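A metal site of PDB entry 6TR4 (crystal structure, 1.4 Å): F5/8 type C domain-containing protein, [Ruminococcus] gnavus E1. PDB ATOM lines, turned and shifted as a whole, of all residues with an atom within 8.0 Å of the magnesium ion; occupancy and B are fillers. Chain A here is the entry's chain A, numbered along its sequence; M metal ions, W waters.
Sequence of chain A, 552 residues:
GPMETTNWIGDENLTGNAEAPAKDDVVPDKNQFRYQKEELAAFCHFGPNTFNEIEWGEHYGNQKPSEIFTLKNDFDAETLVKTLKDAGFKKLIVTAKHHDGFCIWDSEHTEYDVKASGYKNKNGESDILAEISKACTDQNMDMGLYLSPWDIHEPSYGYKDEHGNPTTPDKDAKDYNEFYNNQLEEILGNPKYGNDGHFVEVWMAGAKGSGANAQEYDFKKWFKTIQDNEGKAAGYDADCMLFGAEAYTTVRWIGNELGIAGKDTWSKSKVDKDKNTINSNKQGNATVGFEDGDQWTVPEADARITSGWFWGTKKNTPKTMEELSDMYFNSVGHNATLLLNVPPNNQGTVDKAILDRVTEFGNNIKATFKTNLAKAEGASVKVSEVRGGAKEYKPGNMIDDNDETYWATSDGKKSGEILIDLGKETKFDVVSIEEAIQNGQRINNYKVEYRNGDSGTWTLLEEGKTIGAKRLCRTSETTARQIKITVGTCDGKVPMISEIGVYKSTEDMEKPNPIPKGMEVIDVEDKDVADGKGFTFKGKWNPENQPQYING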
ATOM      1  N   LEU A  71     -33.046   3.754 -19.509  1.00  0.00           N
ATOM      2  CA  LEU A  71     -31.808   4.349 -18.951  1.00  0.00           C
ATOM      3  C   LEU A  71     -32.001   5.859 -18.744  1.00  0.00           C
ATOM      4  O   LEU A  71     -32.335   6.542 -19.733  1.00  0.00           O
ATOM      5  CB  LEU A  71     -30.637   4.072 -19.910  1.00  0.00           C
ATOM      6  CG  LEU A  71     -29.303   4.700 -19.508  1.00  0.00           C
ATOM      7  CD1 LEU A  71     -28.851   4.183 -18.132  1.00  0.00           C
ATOM      8  CD2 LEU A  71     -28.253   4.434 -20.574  1.00  0.00           C
ATOM      9  N   ASN A  73     -29.594   7.861 -16.940  1.00  0.00           N
ATOM     10  CA  ASN A  73     -28.258   8.503 -16.743  1.00  0.00           C
ATOM     11  C   ASN A  73     -27.450   8.348 -18.012  1.00  0.00           C
ATOM     12  O   ASN A  73     -27.595   7.346 -18.719  1.00  0.00           O
ATOM     13  CB  ASN A  73     -27.455   7.861 -15.615  1.00  0.00           C
ATOM     14  CG  ASN A  73     -28.205   7.798 -14.311  1.00  0.00           C
ATOM     15  OD1 ASN A  73     -28.904   8.745 -13.945  1.00  0.00           O
ATOM     16  ND2 ASN A  73     -28.050   6.697 -13.602  1.00  0.00           N
ATOM     17  N   ASP A  74     -26.541   9.281 -18.246  1.00  0.00           N
ATOM     18  CA  ASP A  74     -25.574   9.164 -19.350  1.00  0.00           C
ATOM     19  C   ASP A  74     -24.780   7.857 -19.161  1.00  0.00           C
ATOM     20  O   ASP A  74     -24.223   7.637 -18.076  1.00  0.00           O
ATOM     21  CB  ASP A  74     -24.678  10.393 -19.370  1.00  0.00           C
ATOM     22  CG  ASP A  74     -23.684  10.441 -20.503  1.00  0.00           C
ATOM     23  OD1 ASP A  74     -23.324   9.356 -21.011  1.00  0.00           O
ATOM     24  OD2 ASP A  74     -23.266  11.576 -20.868  1.00  0.00           O
ATOM     25  N   PHE A  75     -24.753   7.012 -20.184  1.00  0.00           N
ATOM     26  CA  PHE A  75     -23.991   5.734 -20.165  1.00  0.00           C
ATOM     27  C   PHE A  75     -22.508   6.019 -19.885  1.00  0.00           C
ATOM     28  O   PHE A  75     -21.896   6.866 -20.576  1.00  0.00           O
ATOM     29  CB  PHE A  75     -24.179   5.024 -21.494  1.00  0.00           C
ATOM     30  CG  PHE A  75     -23.574   3.652 -21.480  1.00  0.00           C
ATOM     31  CD1 PHE A  75     -24.319   2.580 -21.017  1.00  0.00           C
ATOM     32  CD2 PHE A  75     -22.272   3.440 -21.865  1.00  0.00           C
ATOM     33  CE1 PHE A  75     -23.754   1.315 -20.972  1.00  0.00           C
ATOM     34  CE2 PHE A  75     -21.696   2.180 -21.798  1.00  0.00           C
ATOM     35  CZ  PHE A  75     -22.461   1.122 -21.370  1.00  0.00           C
ATOM     36  N   ASP A  76     -21.926   5.348 -18.890  1.00  0.00           N
ATOM     37  CA  ASP A  76     -20.521   5.584 -18.479  1.00  0.00           C
ATOM     38  C   ASP A  76     -19.585   4.629 -19.224  1.00  0.00           C
ATOM     39  O   ASP A  76     -19.099   3.661 -18.647  1.00  0.00           O
ATOM     40  CB  ASP A  76     -20.356   5.467 -16.964  1.00  0.00           C
ATOM     41  CG  ASP A  76     -18.964   5.815 -16.509  1.00  0.00           C
ATOM     42  OD1 ASP A  76     -18.120   6.180 -17.365  1.00  0.00           O
ATOM     43  OD2 ASP A  76     -18.724   5.715 -15.292  1.00  0.00           O
ATOM     44  N   ALA A  77     -19.282   4.920 -20.476  1.00  0.00           N
ATOM     45  CA  ALA A  77     -18.373   4.071 -21.258  1.00  0.00           C
ATOM     46  C   ALA A  77     -16.924   4.214 -20.779  1.00  0.00           C
ATOM     47  O   ALA A  77     -16.164   3.259 -20.864  1.00  0.00           O
ATOM     48  CB  ALA A  77     -18.500   4.388 -22.724  1.00  0.00           C
ATOM     49  N   GLU A  78     -16.558   5.391 -20.263  1.00  0.00           N
ATOM     50  CA  GLU A  78     -15.142   5.692 -19.911  1.00  0.00           C
ATOM     51  C   GLU A  78     -14.682   4.782 -18.766  1.00  0.00           C
ATOM     52  O   GLU A  78     -13.581   4.196 -18.861  1.00  0.00           O
ATOM     53  CB  GLU A  78     -15.006   7.184 -19.594  1.00  0.00           C
ATOM     54  CG  GLU A  78     -15.042   8.058 -20.838  1.00  0.00           C
ATOM     55  CD  GLU A  78     -16.373   8.240 -21.569  1.00  0.00           C
ATOM     56  OE1 GLU A  78     -17.458   8.060 -20.956  1.00  0.00           O
ATOM     57  OE2 GLU A  78     -16.322   8.597 -22.777  1.00  0.00           O
ATOM     58  N   TYR A 119     -33.715   8.057 -24.479  1.00  0.00           N
ATOM     59  CA  TYR A 119     -32.362   8.202 -23.900  1.00  0.00           C
ATOM     60  C   TYR A 119     -31.619   9.339 -24.605  1.00  0.00           C
ATOM     61  O   TYR A 119     -31.639   9.372 -25.839  1.00  0.00           O
ATOM     62  CB  TYR A 119     -31.537   6.918 -24.076  1.00  0.00           C
ATOM     63  CG  TYR A 119     -30.095   7.125 -23.698  1.00  0.00           C
ATOM     64  CD1 TYR A 119     -29.718   7.289 -22.379  1.00  0.00           C
ATOM     65  CD2 TYR A 119     -29.111   7.239 -24.669  1.00  0.00           C
ATOM     66  CE1 TYR A 119     -28.388   7.492 -22.023  1.00  0.00           C
ATOM     67  CE2 TYR A 119     -27.790   7.510 -24.333  1.00  0.00           C
ATOM     68  CZ  TYR A 119     -27.424   7.609 -23.006  1.00  0.00           C
ATOM     69  OH  TYR A 119     -26.116   7.816 -22.654  1.00  0.00           O
ATOM     70  N   LYS A 120     -30.956  10.203 -23.842  1.00  0.00           N
ATOM     71  CA  LYS A 120     -29.990  11.218 -24.354  1.00  0.00           C
ATOM     72  C   LYS A 120     -28.813  11.338 -23.385  1.00  0.00           C
ATOM     73  O   LYS A 120     -29.042  11.304 -22.169  1.00  0.00           O
ATOM     74  CB  LYS A 120     -30.642  12.594 -24.495  1.00  0.00           C
ATOM     75  CG  LYS A 120     -31.791  12.678 -25.477  1.00  0.00           C
ATOM     76  CD  LYS A 120     -32.318  14.098 -25.630  1.00  0.00           C
ATOM     77  CE  LYS A 120     -33.394  14.211 -26.678  1.00  0.00           C
ATOM     78  NZ  LYS A 120     -32.846  14.084 -28.051  1.00  0.00           N
ATOM     79  N   ASN A 121     -27.604  11.504 -23.911  1.00  0.00           N
ATOM     80  CA  ASN A 121     -26.392  11.717 -23.083  1.00  0.00           C
ATOM     81  C   ASN A 121     -26.248  13.216 -22.776  1.00  0.00           C
ATOM     82  O   ASN A 121     -27.136  13.982 -23.178  1.00  0.00           O
ATOM     83  CB  ASN A 121     -25.155  11.091 -23.725  1.00  0.00           C
ATOM     84  CG  ASN A 121     -24.586  11.888 -24.872  1.00  0.00           C
ATOM     85  OD1 ASN A 121     -25.180  12.841 -25.347  1.00  0.00           O
ATOM     86  ND2 ASN A 121     -23.402  11.486 -25.316  1.00  0.00           N
ATOM     87  N   LYS A 122     -25.170  13.588 -22.065  1.00  0.00           N
ATOM     88  CA  LYS A 122     -24.923  14.988 -21.642  1.00  0.00           C
ATOM     89  C   LYS A 122     -24.978  15.927 -22.867  1.00  0.00           C
ATOM     90  O   LYS A 122     -25.408  17.076 -22.700  1.00  0.00           O
ATOM     91  CB  LYS A 122     -23.585  15.091 -20.897  1.00  0.00           C
ATOM     92  CG  LYS A 122     -22.360  14.618 -21.662  1.00  0.00           C
ATOM     93  CD  LYS A 122     -21.048  14.778 -20.897  1.00  0.00           C
ATOM     94  CE  LYS A 122     -19.908  14.025 -21.533  1.00  0.00           C
ATOM     95  NZ  LYS A 122     -18.667  14.103 -20.715  1.00  0.00           N
ATOM     96  N   ASN A 123     -24.558  15.430 -24.043  1.00  0.00           N
ATOM     97  CA  ASN A 123     -24.418  16.194 -25.315  1.00  0.00           C
ATOM     98  C   ASN A 123     -25.662  16.078 -26.190  1.00  0.00           C
ATOM     99  O   ASN A 123     -25.612  16.513 -27.357  1.00  0.00           O
ATOM    100  CB  ASN A 123     -23.196  15.710 -26.109  1.00  0.00           C
ATOM    101  CG  ASN A 123     -21.880  15.865 -25.373  1.00  0.00           C
ATOM    102  OD1 ASN A 123     -21.704  16.821 -24.616  1.00  0.00           O
ATOM    103  ND2 ASN A 123     -20.953  14.953 -25.617  1.00  0.00           N
ATOM    104  N   ASP A 127     -27.001   7.363 -28.741  1.00  0.00           N
ATOM    105  CA  ASP A 127     -26.285   6.286 -29.474  1.00  0.00           C
ATOM    106  C   ASP A 127     -25.254   5.663 -28.526  1.00  0.00           C
ATOM    107  O   ASP A 127     -24.137   6.191 -28.410  1.00  0.00           O
ATOM    108  CB  ASP A 127     -25.690   6.843 -30.759  1.00  0.00           C
ATOM    109  CG  ASP A 127     -25.265   5.726 -31.692  1.00  0.00           C
ATOM    110  OD1 ASP A 127     -24.738   4.723 -31.197  1.00  0.00           O
ATOM    111  OD2 ASP A 127     -25.574   5.854 -32.900  1.00  0.00           O
ATOM    112  N   ILE A 128     -25.643   4.582 -27.860  1.00  0.00           N
ATOM    113  CA  ILE A 128     -24.765   3.902 -26.862  1.00  0.00           C
ATOM    114  C   ILE A 128     -23.559   3.307 -27.613  1.00  0.00           C
ATOM    115  O   ILE A 128     -22.433   3.383 -27.101  1.00  0.00           O
ATOM    116  CB  ILE A 128     -25.475   2.782 -26.074  1.00  0.00           C
ATOM    117  CG1 ILE A 128     -26.792   3.179 -25.441  1.00  0.00           C
ATOM    118  CG2 ILE A 128     -24.548   2.217 -25.024  1.00  0.00           C
ATOM    119  CD1 ILE A 128     -26.657   4.145 -24.335  1.00  0.00           C
ATOM    120  N   ALA A 130     -22.063   4.400 -30.257  1.00  0.00           N
ATOM    121  CA  ALA A 130     -21.113   5.514 -30.520  1.00  0.00           C
ATOM    122  C   ALA A 130     -20.395   5.921 -29.234  1.00  0.00           C
ATOM    123  O   ALA A 130     -19.185   6.159 -29.272  1.00  0.00           O
ATOM    124  CB  ALA A 130     -21.809   6.675 -31.155  1.00  0.00           C
ATOM    125  N   GLU A 131     -21.095   5.963 -28.101  1.00  0.00           N
ATOM    126  CA  GLU A 131     -20.412   6.371 -26.829  1.00  0.00           C
ATOM    127  C   GLU A 131     -19.338   5.349 -26.474  1.00  0.00           C
ATOM    128  O   GLU A 131     -18.231   5.711 -26.063  1.00  0.00           O
ATOM    129  CB  GLU A 131     -21.393   6.452 -25.661  1.00  0.00           C
ATOM    130  CG  GLU A 131     -22.355   7.602 -25.726  1.00  0.00           C
ATOM    131  CD  GLU A 131     -23.280   7.668 -24.519  1.00  0.00           C
ATOM    132  OE1 GLU A 131     -22.763   7.630 -23.381  1.00  0.00           O
ATOM    133  OE2 GLU A 131     -24.483   7.815 -24.714  1.00  0.00           O
ATOM    134  N   ILE A 132     -19.639   4.067 -26.584  1.00  0.00           N
ATOM    135  CA  ILE A 132     -18.643   3.014 -26.274  1.00  0.00           C
ATOM    136  C   ILE A 132     -17.482   3.119 -27.274  1.00  0.00           C
ATOM    137  O   ILE A 132     -16.343   3.018 -26.849  1.00  0.00           O
ATOM    138  CB  ILE A 132     -19.293   1.625 -26.246  1.00  0.00           C
ATOM    139  CG1 ILE A 132     -20.353   1.550 -25.137  1.00  0.00           C
ATOM    140  CG2 ILE A 132     -18.239   0.561 -26.070  1.00  0.00           C
ATOM    141  CD1 ILE A 132     -21.203   0.284 -25.168  1.00  0.00           C
ATOM    142  N   ALA A 135     -15.088   5.944 -26.341  1.00  0.00           N
ATOM    143  CA  ALA A 135     -14.243   5.571 -25.183  1.00  0.00           C
ATOM    144  C   ALA A 135     -13.169   4.564 -25.621  1.00  0.00           C
ATOM    145  O   ALA A 135     -11.987   4.667 -25.218  1.00  0.00           O
ATOM    146  CB  ALA A 135     -15.103   5.030 -24.092  1.00  0.00           C
ATOM    147  N   GLY A 348     -26.462   2.505 -16.184  1.00  0.00           N
ATOM    148  CA  GLY A 348     -25.494   2.802 -17.271  1.00  0.00           C
ATOM    149  C   GLY A 348     -24.055   2.815 -16.787  1.00  0.00           C
ATOM    150  O   GLY A 348     -23.178   3.233 -17.556  1.00  0.00           O
HETATM  151 MG    MG M   1     -21.599   8.502 -21.843  1.00  0.00          MG
HETATM  152  O   HOH W   1     -20.530   9.402 -20.177  1.00  0.00           O
HETATM  153  O   HOH W   2     -19.672   7.726 -22.327  1.00  0.00           O
HETATM  154  O   HOH W   3     -21.358  10.299 -22.994  1.00  0.00           O
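The side-chain carboxylate (OE2) of Glu 131 is in hydrogen-bond range of the side-chain hydroxyl (OH) of Tyr 119.
The side-chain carboxylate (OD2) of Asp 74 sits at hydrogen-bond distance from the backbone NH (N) of Lys 122.
The side-chain hydroxyl of Tyr 119 is in hydrogen-bond range of the backbone NH of Phe 75, at 2.9 Å.
The magnesium ion is bound by O of Phe 75 (2.1 Å), OD1 of Asp 74 (2.1 Å), OE1 of Glu 131 (2.1 Å), water W2 (2.1 Å), water W3 (2.1 Å) and water W1 (2.2 Å).
Water W3 bridges OD2 of Asp 74 and ND2 of Asn 121.
Water W2 bridges OE1 of Glu 78 (2.6 Å) and N of Ala 77 (3.4 Å).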
